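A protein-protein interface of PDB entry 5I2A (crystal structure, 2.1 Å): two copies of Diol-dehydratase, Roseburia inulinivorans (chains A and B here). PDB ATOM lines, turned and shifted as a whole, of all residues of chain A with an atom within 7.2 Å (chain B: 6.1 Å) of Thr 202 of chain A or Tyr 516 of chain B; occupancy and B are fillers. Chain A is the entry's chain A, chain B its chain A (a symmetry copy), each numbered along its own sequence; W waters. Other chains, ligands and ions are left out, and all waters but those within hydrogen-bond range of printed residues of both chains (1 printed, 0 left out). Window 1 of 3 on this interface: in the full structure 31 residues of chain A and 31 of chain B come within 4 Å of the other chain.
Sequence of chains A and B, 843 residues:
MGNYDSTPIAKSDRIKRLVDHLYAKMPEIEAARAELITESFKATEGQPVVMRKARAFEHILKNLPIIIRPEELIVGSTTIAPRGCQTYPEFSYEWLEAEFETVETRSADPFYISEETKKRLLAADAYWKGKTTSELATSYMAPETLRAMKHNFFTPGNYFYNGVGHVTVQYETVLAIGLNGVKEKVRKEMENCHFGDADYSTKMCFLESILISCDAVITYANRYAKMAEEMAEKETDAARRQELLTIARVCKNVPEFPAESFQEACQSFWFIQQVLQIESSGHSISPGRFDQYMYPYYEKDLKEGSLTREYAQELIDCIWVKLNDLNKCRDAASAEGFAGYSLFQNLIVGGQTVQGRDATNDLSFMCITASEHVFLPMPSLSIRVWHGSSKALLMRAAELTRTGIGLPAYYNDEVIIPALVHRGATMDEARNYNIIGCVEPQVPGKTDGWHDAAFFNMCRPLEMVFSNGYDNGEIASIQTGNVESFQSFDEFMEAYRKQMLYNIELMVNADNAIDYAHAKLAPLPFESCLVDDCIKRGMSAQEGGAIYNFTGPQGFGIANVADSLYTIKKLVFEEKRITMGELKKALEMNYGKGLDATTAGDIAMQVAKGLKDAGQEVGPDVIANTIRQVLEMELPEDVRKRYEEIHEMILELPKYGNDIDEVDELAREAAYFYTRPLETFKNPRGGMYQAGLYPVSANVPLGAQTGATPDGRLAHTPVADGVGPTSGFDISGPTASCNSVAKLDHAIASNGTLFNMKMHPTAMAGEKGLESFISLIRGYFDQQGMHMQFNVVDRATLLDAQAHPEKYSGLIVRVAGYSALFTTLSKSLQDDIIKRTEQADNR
O of Ala 198 of chain A lies within hydrogen-bond range of OH of Tyr 516 of chain B, at 2.6 Å.
The backbone carbonyl oxygen (O) of Tyr 140 of chain B sits at hydrogen-bond distance from the side-chain hydroxyl (OG) of Ser 201 of chain A (2.9 Å).
The side-chain hydroxyl of Thr 202 of chain A is in hydrogen-bond range of the backbone carbonyl oxygen of Asp 199 of chain A, at 3.3 Å.
CD1 of Leu 136 of chain B touches N of Pro 48 of chain A (3.6 Å).
Pro 48 of chain A touches Tyr 140 of chain B (CG to CE1, 3.5 Å).
Asn 512 of chain B touches Asp 197 of chain A (ND2 to O, 3.8 Å).
Ala 198 of chain A touches Asn 512 of chain B (CA to ND2, 3.9 Å).
CG of Pro 684 of chain B touches O of Ala 198 of chain A, at 3.8 Å.
CA of Asp 199 of chain A touches OH of Tyr 516 of chain B, 3.4 Å away.
OG of Ser 201 of chain A touches CA of Ala 513 of chain B, 3.7 Å away.
Ser 201 of chain A touches Tyr 516 of chain B.
Thr 202 of chain A touches Tyr 140 of chain B.
CG2 of Thr 202 of chain A touches CE1 of Tyr 516 of chain B (3.7 Å).
Of the printed residues of chain B, Asp 197 of chain A touches Asn 512.
Of the printed residues of chain B, Asp 199 of chain A touches Tyr 516.
Of the printed residues of chain B, Ser 201 of chain A touches Tyr 140 (2.9 Å), Ala 513 (3.7 Å) and Tyr 516 (3.8 Å).
Of chain B, only Tyr 140 and Tyr 516 come within 4 Å of Thr 202 of chain A.
Glu 208 of chain A touches none of the printed residues of chain B.
Of the printed residues of chain A, Asn 512 of chain B touches Asp 197 (3.8 Å) and Ala 198 (3.9 Å).
Printed residues of chain A within 4 Å of Ala 513 of chain B: Ser 201 (3.7 Å).
Ile 514 of chain B touches none of the printed residues of chain A.
Tyr 516 of chain B touches just these residues of chain A: Ala 198, Asp 199, Ser 201 and Thr 202.
The nearest residue of chain B that does not touch Thr 202 of chain A is Lys 520 of chain B (4.3 Å).
The nearest residue of chain A that does not touch Tyr 516 of chain B is Tyr 200 of chain A (5.0 Å).
The nearest printed residue of chain A that does not touch Ala 513 of chain B is Ala 198 of chain A (7.1 Å).
Hydrophobic or aromatic side chains of chain B within 4 Å of the printed part of chain A: Leu 136, Tyr 140, Ala 513, Tyr 516 and Pro 684.
Among the printed residues, no Asp or Glu carboxylate lies within 4 Å of a Lys or Arg side-chain nitrogen of the other chain.
No position is printed for both chains.
Of the 12 pairs that touch across the chains among the printed residues, none has its exchanged pair printed and touching as well.
Water W1 lies within hydrogen-bond range of the backbone carbonyl oxygen of Asp 197 of chain A and the side-chain amide nitrogen of Asn 512 of chain B.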
ATOM      1  N   PRO A  48     -19.272  -2.346 -25.386  1.00  0.00           N
ATOM      2  CA  PRO A  48     -19.440  -2.031 -23.963  1.00  0.00           C
ATOM      3  C   PRO A  48     -19.633  -3.301 -23.141  1.00  0.00           C
ATOM      4  O   PRO A  48     -20.251  -4.254 -23.625  1.00  0.00           O
ATOM      5  CB  PRO A  48     -20.708  -1.170 -23.933  1.00  0.00           C
ATOM      6  CG  PRO A  48     -20.887  -0.686 -25.335  1.00  0.00           C
ATOM      7  CD  PRO A  48     -20.363  -1.779 -26.197  1.00  0.00           C
ATOM      8  N   VAL A  50     -21.549  -4.257 -20.669  1.00  0.00           N
ATOM      9  CA  VAL A  50     -22.850  -4.818 -20.381  1.00  0.00           C
ATOM     10  C   VAL A  50     -23.432  -5.494 -21.632  1.00  0.00           C
ATOM     11  O   VAL A  50     -24.166  -6.474 -21.523  1.00  0.00           O
ATOM     12  CB  VAL A  50     -23.821  -3.755 -19.808  1.00  0.00           C
ATOM     13  CG1 VAL A  50     -24.258  -2.744 -20.870  1.00  0.00           C
ATOM     14  CG2 VAL A  50     -25.028  -4.439 -19.196  1.00  0.00           C
ATOM     15  N   ASP A 197     -29.541  13.066 -25.039  1.00  0.00           N
ATOM     16  CA  ASP A 197     -29.463  12.971 -23.573  1.00  0.00           C
ATOM     17  C   ASP A 197     -28.034  12.593 -23.174  1.00  0.00           C
ATOM     18  O   ASP A 197     -27.422  11.757 -23.817  1.00  0.00           O
ATOM     19  CB  ASP A 197     -30.443  11.922 -23.004  1.00  0.00           C
ATOM     20  CG  ASP A 197     -31.909  12.267 -23.265  1.00  0.00           C
ATOM     21  OD1 ASP A 197     -32.211  13.426 -23.596  1.00  0.00           O
ATOM     22  OD2 ASP A 197     -32.755  11.362 -23.157  1.00  0.00           O
ATOM     23  N   ALA A 198     -27.520  13.202 -22.112  1.00  0.00           N
ATOM     24  CA  ALA A 198     -26.159  12.932 -21.659  1.00  0.00           C
ATOM     25  C   ALA A 198     -25.940  11.460 -21.297  1.00  0.00           C
ATOM     26  O   ALA A 198     -24.817  10.970 -21.379  1.00  0.00           O
ATOM     27  CB  ALA A 198     -25.798  13.839 -20.461  1.00  0.00           C
ATOM     28  N   ASP A 199     -26.998  10.744 -20.924  1.00  0.00           N
ATOM     29  CA  ASP A 199     -26.840   9.324 -20.592  1.00  0.00           C
ATOM     30  C   ASP A 199     -27.395   8.376 -21.662  1.00  0.00           C
ATOM     31  O   ASP A 199     -27.593   7.189 -21.391  1.00  0.00           O
ATOM     32  CB  ASP A 199     -27.511   9.013 -19.234  1.00  0.00           C
ATOM     33  CG  ASP A 199     -29.022   9.110 -19.296  1.00  0.00           C
ATOM     34  OD1 ASP A 199     -29.535   9.814 -20.185  1.00  0.00           O
ATOM     35  OD2 ASP A 199     -29.707   8.479 -18.458  1.00  0.00           O
ATOM     36  N   TYR A 200     -27.649   8.881 -22.868  1.00  0.00           N
ATOM     37  CA  TYR A 200     -28.310   8.057 -23.880  1.00  0.00           C
ATOM     38  C   TYR A 200     -27.475   6.821 -24.236  1.00  0.00           C
ATOM     39  O   TYR A 200     -28.003   5.714 -24.266  1.00  0.00           O
ATOM     40  CB  TYR A 200     -28.621   8.861 -25.145  1.00  0.00           C
ATOM     41  CG  TYR A 200     -29.391   8.073 -26.217  1.00  0.00           C
ATOM     42  CD1 TYR A 200     -28.724   7.293 -27.158  1.00  0.00           C
ATOM     43  CD2 TYR A 200     -30.784   8.118 -26.278  1.00  0.00           C
ATOM     44  CE1 TYR A 200     -29.424   6.577 -28.136  1.00  0.00           C
ATOM     45  CE2 TYR A 200     -31.489   7.426 -27.249  1.00  0.00           C
ATOM     46  CZ  TYR A 200     -30.807   6.660 -28.176  1.00  0.00           C
ATOM     47  OH  TYR A 200     -31.508   5.967 -29.119  1.00  0.00           O
ATOM     48  N   SER A 201     -26.180   6.999 -24.479  1.00  0.00           N
ATOM     49  CA  SER A 201     -25.349   5.870 -24.906  1.00  0.00           C
ATOM     50  C   SER A 201     -25.380   4.700 -23.908  1.00  0.00           C
ATOM     51  O   SER A 201     -25.536   3.543 -24.293  1.00  0.00           O
ATOM     52  CB  SER A 201     -23.900   6.307 -25.125  1.00  0.00           C
ATOM     53  OG  SER A 201     -23.758   7.106 -26.285  1.00  0.00           O
ATOM     54  N   THR A 202     -25.217   5.010 -22.632  1.00  0.00           N
ATOM     55  CA  THR A 202     -25.091   3.981 -21.617  1.00  0.00           C
ATOM     56  C   THR A 202     -26.457   3.429 -21.206  1.00  0.00           C
ATOM     57  O   THR A 202     -26.600   2.232 -20.983  1.00  0.00           O
ATOM     58  CB  THR A 202     -24.359   4.517 -20.371  1.00  0.00           C
ATOM     59  OG1 THR A 202     -24.970   5.748 -19.956  1.00  0.00           O
ATOM     60  CG2 THR A 202     -22.857   4.752 -20.684  1.00  0.00           C
ATOM     61  N   LYS A 203     -27.457   4.302 -21.104  1.00  0.00           N
ATOM     62  CA  LYS A 203     -28.803   3.855 -20.764  1.00  0.00           C
ATOM     63  C   LYS A 203     -29.330   2.926 -21.851  1.00  0.00           C
ATOM     64  O   LYS A 203     -29.842   1.841 -21.562  1.00  0.00           O
ATOM     65  CB  LYS A 203     -29.766   5.039 -20.562  1.00  0.00           C
ATOM     66  CG  LYS A 203     -31.224   4.622 -20.331  1.00  0.00           C
ATOM     67  CD  LYS A 203     -32.059   5.718 -19.647  1.00  0.00           C
ATOM     68  CE  LYS A 203     -33.449   5.190 -19.245  1.00  0.00           C
ATOM     69  NZ  LYS A 203     -34.335   6.241 -18.638  1.00  0.00           N
ATOM     70  N   MET A 204     -29.200   3.346 -23.103  1.00  0.00           N
ATOM     71  CA  MET A 204     -29.763   2.571 -24.202  1.00  0.00           C
ATOM     72  C   MET A 204     -29.003   1.273 -24.391  1.00  0.00           C
ATOM     73  O   MET A 204     -29.608   0.266 -24.698  1.00  0.00           O
ATOM     74  CB  MET A 204     -29.775   3.375 -25.502  1.00  0.00           C
ATOM     75  CG  MET A 204     -30.855   4.457 -25.539  1.00  0.00           C
ATOM     76  SD  MET A 204     -32.531   3.749 -25.504  1.00  0.00           S
ATOM     77  CE  MET A 204     -32.352   2.547 -26.802  1.00  0.00           C
ATOM     78  N   CYS A 205     -27.685   1.282 -24.188  1.00  0.00           N
ATOM     79  CA  CYS A 205     -26.940   0.029 -24.253  1.00  0.00           C
ATOM     80  C   CYS A 205     -27.467  -0.979 -23.204  1.00  0.00           C
ATOM     81  O   CYS A 205     -27.644  -2.153 -23.501  1.00  0.00           O
ATOM     82  CB  CYS A 205     -25.443   0.260 -24.051  1.00  0.00           C
ATOM     83  SG  CYS A 205     -24.413  -1.205 -24.368  1.00  0.00           S
ATOM     84  N   PHE A 206     -27.696  -0.512 -21.982  1.00  0.00           N
ATOM     85  CA  PHE A 206     -28.204  -1.370 -20.910  1.00  0.00           C
ATOM     86  C   PHE A 206     -29.594  -1.908 -21.254  1.00  0.00           C
ATOM     87  O   PHE A 206     -29.852  -3.098 -21.116  1.00  0.00           O
ATOM     88  CB  PHE A 206     -28.240  -0.609 -19.582  1.00  0.00           C
ATOM     89  CG  PHE A 206     -28.887  -1.366 -18.466  1.00  0.00           C
ATOM     90  CD1 PHE A 206     -28.273  -2.476 -17.909  1.00  0.00           C
ATOM     91  CD2 PHE A 206     -30.122  -0.971 -17.972  1.00  0.00           C
ATOM     92  CE1 PHE A 206     -28.882  -3.181 -16.877  1.00  0.00           C
ATOM     93  CE2 PHE A 206     -30.728  -1.666 -16.938  1.00  0.00           C
ATOM     94  CZ  PHE A 206     -30.110  -2.776 -16.395  1.00  0.00           C
ATOM     95  N   LEU A 207     -30.476  -1.028 -21.723  1.00  0.00           N
ATOM     96  CA  LEU A 207     -31.823  -1.440 -22.116  1.00  0.00           C
ATOM     97  C   LEU A 207     -31.781  -2.451 -23.279  1.00  0.00           C
ATOM     98  O   LEU A 207     -32.510  -3.430 -23.253  1.00  0.00           O
ATOM     99  CB  LEU A 207     -32.686  -0.220 -22.477  1.00  0.00           C
ATOM    100  CG  LEU A 207     -32.969   0.755 -21.316  1.00  0.00           C
ATOM    101  CD1 LEU A 207     -33.825   1.942 -21.737  1.00  0.00           C
ATOM    102  CD2 LEU A 207     -33.626   0.035 -20.138  1.00  0.00           C
ATOM    103  N   GLU A 208     -30.923  -2.237 -24.279  1.00  0.00           N
ATOM    104  CA  GLU A 208     -30.812  -3.203 -25.377  1.00  0.00           C
ATOM    105  C   GLU A 208     -30.303  -4.538 -24.862  1.00  0.00           C
ATOM    106  O   GLU A 208     -30.724  -5.588 -25.333  1.00  0.00           O
ATOM    107  CB  GLU A 208     -29.873  -2.717 -26.483  1.00  0.00           C
ATOM    108  CG  GLU A 208     -30.256  -1.401 -27.127  1.00  0.00           C
ATOM    109  CD  GLU A 208     -31.275  -1.545 -28.235  1.00  0.00           C
ATOM    110  OE1 GLU A 208     -31.870  -2.640 -28.382  1.00  0.00           O
ATOM    111  OE2 GLU A 208     -31.470  -0.550 -28.972  1.00  0.00           O
ATOM    112  N   GLY A 538     -31.712   3.064 -16.016  1.00  0.00           N
ATOM    113  CA  GLY A 538     -30.824   2.736 -17.105  1.00  0.00           C
ATOM    114  C   GLY A 538     -29.483   2.180 -16.658  1.00  0.00           C
ATOM    115  O   GLY A 538     -28.495   2.346 -17.356  1.00  0.00           O
ATOM    116  N   MET A 539     -29.444   1.527 -15.500  1.00  0.00           N
ATOM    117  CA  MET A 539     -28.198   0.924 -15.018  1.00  0.00           C
ATOM    118  C   MET A 539     -28.465  -0.376 -14.271  1.00  0.00           C
ATOM    119  O   MET A 539     -29.530  -0.569 -13.713  1.00  0.00           O
ATOM    120  CB  MET A 539     -27.430   1.893 -14.115  1.00  0.00           C
ATOM    121  CG  MET A 539     -28.259   2.428 -12.957  1.00  0.00           C
ATOM    122  SD  MET A 539     -27.699   4.056 -12.467  1.00  0.00           S
ATOM    123  CE  MET A 539     -26.592   3.633 -11.137  1.00  0.00           C
ATOM    124  N   GLU A 543     -24.492  -1.613 -10.415  1.00  0.00           N
ATOM    125  CA  GLU A 543     -24.037  -0.220 -10.516  1.00  0.00           C
ATOM    126  C   GLU A 543     -24.819   0.795  -9.678  1.00  0.00           C
ATOM    127  O   GLU A 543     -24.445   1.956  -9.636  1.00  0.00           O
ATOM    128  CB  GLU A 543     -24.098   0.251 -11.977  1.00  0.00           C
ATOM    129  CG  GLU A 543     -23.110  -0.443 -12.868  1.00  0.00           C
ATOM    130  CD  GLU A 543     -23.436  -0.241 -14.321  1.00  0.00           C
ATOM    131  OE1 GLU A 543     -24.398  -0.869 -14.812  1.00  0.00           O
ATOM    132  OE2 GLU A 543     -22.736   0.560 -14.966  1.00  0.00           O
ATOM    133  N   LEU B 136     -14.938   1.352 -29.047  1.00  0.00           N
ATOM    134  CA  LEU B 136     -15.966   1.523 -28.022  1.00  0.00           C
ATOM    135  C   LEU B 136     -16.900   2.686 -28.372  1.00  0.00           C
ATOM    136  O   LEU B 136     -18.110   2.576 -28.227  1.00  0.00           O
ATOM    137  CB  LEU B 136     -15.332   1.739 -26.645  1.00  0.00           C
ATOM    138  CG  LEU B 136     -16.314   1.893 -25.482  1.00  0.00           C
ATOM    139  CD1 LEU B 136     -17.225   0.662 -25.393  1.00  0.00           C
ATOM    140  CD2 LEU B 136     -15.576   2.108 -24.154  1.00  0.00           C
ATOM    141  N   TYR B 140     -21.173   2.791 -29.110  1.00  0.00           N
ATOM    142  CA  TYR B 140     -22.063   3.640 -28.318  1.00  0.00           C
ATOM    143  C   TYR B 140     -22.886   4.632 -29.161  1.00  0.00           C
ATOM    144  O   TYR B 140     -23.678   5.387 -28.614  1.00  0.00           O
ATOM    145  CB  TYR B 140     -21.263   4.413 -27.268  1.00  0.00           C
ATOM    146  CG  TYR B 140     -21.087   3.722 -25.934  1.00  0.00           C
ATOM    147  CD1 TYR B 140     -22.143   3.041 -25.317  1.00  0.00           C
ATOM    148  CD2 TYR B 140     -19.870   3.786 -25.266  1.00  0.00           C
ATOM    149  CE1 TYR B 140     -21.970   2.442 -24.071  1.00  0.00           C
ATOM    150  CE2 TYR B 140     -19.689   3.186 -24.041  1.00  0.00           C
ATOM    151  CZ  TYR B 140     -20.730   2.521 -23.441  1.00  0.00           C
ATOM    152  OH  TYR B 140     -20.505   1.955 -22.203  1.00  0.00           O
ATOM    153  N   TRP B 450     -13.287  20.363 -24.653  1.00  0.00           N
ATOM    154  CA  TRP B 450     -13.610  19.631 -25.889  1.00  0.00           C
ATOM    155  C   TRP B 450     -13.803  20.625 -27.030  1.00  0.00           C
ATOM    156  O   TRP B 450     -14.782  20.565 -27.769  1.00  0.00           O
ATOM    157  CB  TRP B 450     -14.860  18.750 -25.682  1.00  0.00           C
ATOM    158  CG  TRP B 450     -14.511  17.348 -25.217  1.00  0.00           C
ATOM    159  CD1 TRP B 450     -13.701  17.012 -24.174  1.00  0.00           C
ATOM    160  CD2 TRP B 450     -14.960  16.110 -25.789  1.00  0.00           C
ATOM    161  NE1 TRP B 450     -13.607  15.656 -24.066  1.00  0.00           N
ATOM    162  CE2 TRP B 450     -14.368  15.073 -25.046  1.00  0.00           C
ATOM    163  CE3 TRP B 450     -15.807  15.782 -26.854  1.00  0.00           C
ATOM    164  CZ2 TRP B 450     -14.594  13.721 -25.328  1.00  0.00           C
ATOM    165  CZ3 TRP B 450     -16.030  14.434 -27.143  1.00  0.00           C
ATOM    166  CH2 TRP B 450     -15.414  13.424 -26.392  1.00  0.00           C
ATOM    167  N   ASP B 511     -20.657  12.786 -30.270  1.00  0.00           N
ATOM    168  CA  ASP B 511     -19.646  13.302 -29.353  1.00  0.00           C
ATOM    169  C   ASP B 511     -19.789  12.694 -27.954  1.00  0.00           C
ATOM    170  O   ASP B 511     -18.795  12.345 -27.330  1.00  0.00           O
ATOM    171  CB  ASP B 511     -19.717  14.832 -29.270  1.00  0.00           C
ATOM    172  CG  ASP B 511     -18.968  15.507 -30.389  1.00  0.00           C
ATOM    173  OD1 ASP B 511     -17.935  14.957 -30.839  1.00  0.00           O
ATOM    174  OD2 ASP B 511     -19.400  16.593 -30.805  1.00  0.00           O
ATOM    175  N   ASN B 512     -21.022  12.572 -27.473  1.00  0.00           N
ATOM    176  CA  ASN B 512     -21.252  11.975 -26.159  1.00  0.00           C
ATOM    177  C   ASN B 512     -20.788  10.512 -26.144  1.00  0.00           C
ATOM    178  O   ASN B 512     -20.227  10.046 -25.163  1.00  0.00           O
ATOM    179  CB  ASN B 512     -22.732  12.087 -25.748  1.00  0.00           C
ATOM    180  CG  ASN B 512     -23.117  13.511 -25.323  1.00  0.00           C
ATOM    181  OD1 ASN B 512     -22.260  14.386 -25.203  1.00  0.00           O
ATOM    182  ND2 ASN B 512     -24.400  13.730 -25.065  1.00  0.00           N
ATOM    183  N   ALA B 513     -21.010   9.800 -27.241  1.00  0.00           N
ATOM    184  CA  ALA B 513     -20.512   8.427 -27.362  1.00  0.00           C
ATOM    185  C   ALA B 513     -18.981   8.369 -27.269  1.00  0.00           C
ATOM    186  O   ALA B 513     -18.424   7.534 -26.564  1.00  0.00           O
ATOM    187  CB  ALA B 513     -20.989   7.798 -28.678  1.00  0.00           C
ATOM    188  N   ILE B 514     -18.308   9.266 -27.978  1.00  0.00           N
ATOM    189  CA  ILE B 514     -16.849   9.325 -27.937  1.00  0.00           C
ATOM    190  C   ILE B 514     -16.367   9.747 -26.534  1.00  0.00           C
ATOM    191  O   ILE B 514     -15.354   9.267 -26.053  1.00  0.00           O
ATOM    192  CB  ILE B 514     -16.325  10.275 -29.032  1.00  0.00           C
ATOM    193  CG1 ILE B 514     -16.689   9.705 -30.408  1.00  0.00           C
ATOM    194  CG2 ILE B 514     -14.800  10.495 -28.920  1.00  0.00           C
ATOM    195  CD1 ILE B 514     -16.563  10.707 -31.570  1.00  0.00           C
ATOM    196  N   ASP B 515     -17.135  10.615 -25.885  1.00  0.00           N
ATOM    197  CA  ASP B 515     -16.877  11.070 -24.517  1.00  0.00           C
ATOM    198  C   ASP B 515     -16.835   9.885 -23.549  1.00  0.00           C
ATOM    199  O   ASP B 515     -15.891   9.744 -22.773  1.00  0.00           O
ATOM    200  CB  ASP B 515     -17.960  12.086 -24.101  1.00  0.00           C
ATOM    201  CG  ASP B 515     -17.441  13.180 -23.150  1.00  0.00           C
ATOM    202  OD1 ASP B 515     -16.498  12.944 -22.364  1.00  0.00           O
ATOM    203  OD2 ASP B 515     -18.021  14.286 -23.179  1.00  0.00           O
ATOM    204  N   TYR B 516     -17.850   9.021 -23.620  1.00  0.00           N
ATOM    205  CA  TYR B 516     -17.872   7.809 -22.806  1.00  0.00           C
ATOM    206  C   TYR B 516     -16.652   6.965 -23.084  1.00  0.00           C
ATOM    207  O   TYR B 516     -16.054   6.450 -22.158  1.00  0.00           O
ATOM    208  CB  TYR B 516     -19.149   6.976 -23.043  1.00  0.00           C
ATOM    209  CG  TYR B 516     -20.313   7.526 -22.265  1.00  0.00           C
ATOM    210  CD1 TYR B 516     -20.291   7.538 -20.866  1.00  0.00           C
ATOM    211  CD2 TYR B 516     -21.405   8.082 -22.913  1.00  0.00           C
ATOM    212  CE1 TYR B 516     -21.340   8.076 -20.133  1.00  0.00           C
ATOM    213  CE2 TYR B 516     -22.459   8.624 -22.194  1.00  0.00           C
ATOM    214  CZ  TYR B 516     -22.423   8.615 -20.807  1.00  0.00           C
ATOM    215  OH  TYR B 516     -23.472   9.146 -20.103  1.00  0.00           O
ATOM    216  N   ALA B 517     -16.269   6.847 -24.355  1.00  0.00           N
ATOM    217  CA  ALA B 517     -15.115   6.015 -24.685  1.00  0.00           C
ATOM    218  C   ALA B 517     -13.831   6.544 -24.021  1.00  0.00           C
ATOM    219  O   ALA B 517     -13.081   5.765 -23.429  1.00  0.00           O
ATOM    220  CB  ALA B 517     -14.936   5.903 -26.207  1.00  0.00           C
ATOM    221  N   HIS B 518     -13.588   7.855 -24.079  1.00  0.00           N
ATOM    222  CA  HIS B 518     -12.413   8.405 -23.391  1.00  0.00           C
ATOM    223  C   HIS B 518     -12.497   8.236 -21.865  1.00  0.00           C
ATOM    224  O   HIS B 518     -11.497   7.906 -21.224  1.00  0.00           O
ATOM    225  CB  HIS B 518     -12.192   9.882 -23.758  1.00  0.00           C
ATOM    226  CG  HIS B 518     -11.642  10.065 -25.144  1.00  0.00           C
ATOM    227  ND1 HIS B 518     -10.309   9.879 -25.445  1.00  0.00           N
ATOM    228  CD2 HIS B 518     -12.252  10.361 -26.316  1.00  0.00           C
ATOM    229  CE1 HIS B 518     -10.123  10.055 -26.739  1.00  0.00           C
ATOM    230  NE2 HIS B 518     -11.283  10.356 -27.291  1.00  0.00           N
ATOM    231  N   ALA B 519     -13.678   8.458 -21.297  1.00  0.00           N
ATOM    232  CA  ALA B 519     -13.875   8.326 -19.855  1.00  0.00           C
ATOM    233  C   ALA B 519     -13.539   6.921 -19.384  1.00  0.00           C
ATOM    234  O   ALA B 519     -12.950   6.746 -18.334  1.00  0.00           O
ATOM    235  CB  ALA B 519     -15.327   8.680 -19.462  1.00  0.00           C
ATOM    236  N   LYS B 520     -13.894   5.924 -20.183  1.00  0.00           N
ATOM    237  CA  LYS B 520     -13.772   4.544 -19.746  1.00  0.00           C
ATOM    238  C   LYS B 520     -12.409   3.956 -20.044  1.00  0.00           C
ATOM    239  O   LYS B 520     -11.894   3.173 -19.265  1.00  0.00           O
ATOM    240  CB  LYS B 520     -14.881   3.695 -20.385  1.00  0.00           C
ATOM    241  CG  LYS B 520     -16.286   4.059 -19.825  1.00  0.00           C
ATOM    242  CD  LYS B 520     -17.405   3.323 -20.534  1.00  0.00           C
ATOM    243  CE  LYS B 520     -18.790   3.632 -19.914  1.00  0.00           C
ATOM    244  NZ  LYS B 520     -18.906   3.150 -18.528  1.00  0.00           N
ATOM    245  N   LEU B 521     -11.809   4.350 -21.159  1.00  0.00           N
ATOM    246  CA  LEU B 521     -10.593   3.690 -21.601  1.00  0.00           C
ATOM    247  C   LEU B 521      -9.346   4.580 -21.575  1.00  0.00           C
ATOM    248  O   LEU B 521      -8.237   4.072 -21.547  1.00  0.00           O
ATOM    249  CB  LEU B 521     -10.801   3.124 -23.014  1.00  0.00           C
ATOM    250  CG  LEU B 521     -11.824   1.984 -23.141  1.00  0.00           C
ATOM    251  CD1 LEU B 521     -11.964   1.521 -24.597  1.00  0.00           C
ATOM    252  CD2 LEU B 521     -11.434   0.801 -22.238  1.00  0.00           C
ATOM    253  N   PRO B 684     -21.436  13.962 -20.919  1.00  0.00           N
ATOM    254  CA  PRO B 684     -21.315  13.034 -19.787  1.00  0.00           C
ATOM    255  C   PRO B 684     -20.354  13.493 -18.700  1.00  0.00           C
ATOM    256  O   PRO B 684     -20.278  12.835 -17.663  1.00  0.00           O
ATOM    257  CB  PRO B 684     -20.792  11.740 -20.442  1.00  0.00           C
ATOM    258  CG  PRO B 684     -21.168  11.871 -21.869  1.00  0.00           C
ATOM    259  CD  PRO B 684     -21.007  13.319 -22.174  1.00  0.00           C
HETATM  260  O   HOH W   1     -26.201  11.679 -26.153  1.00  0.00           O
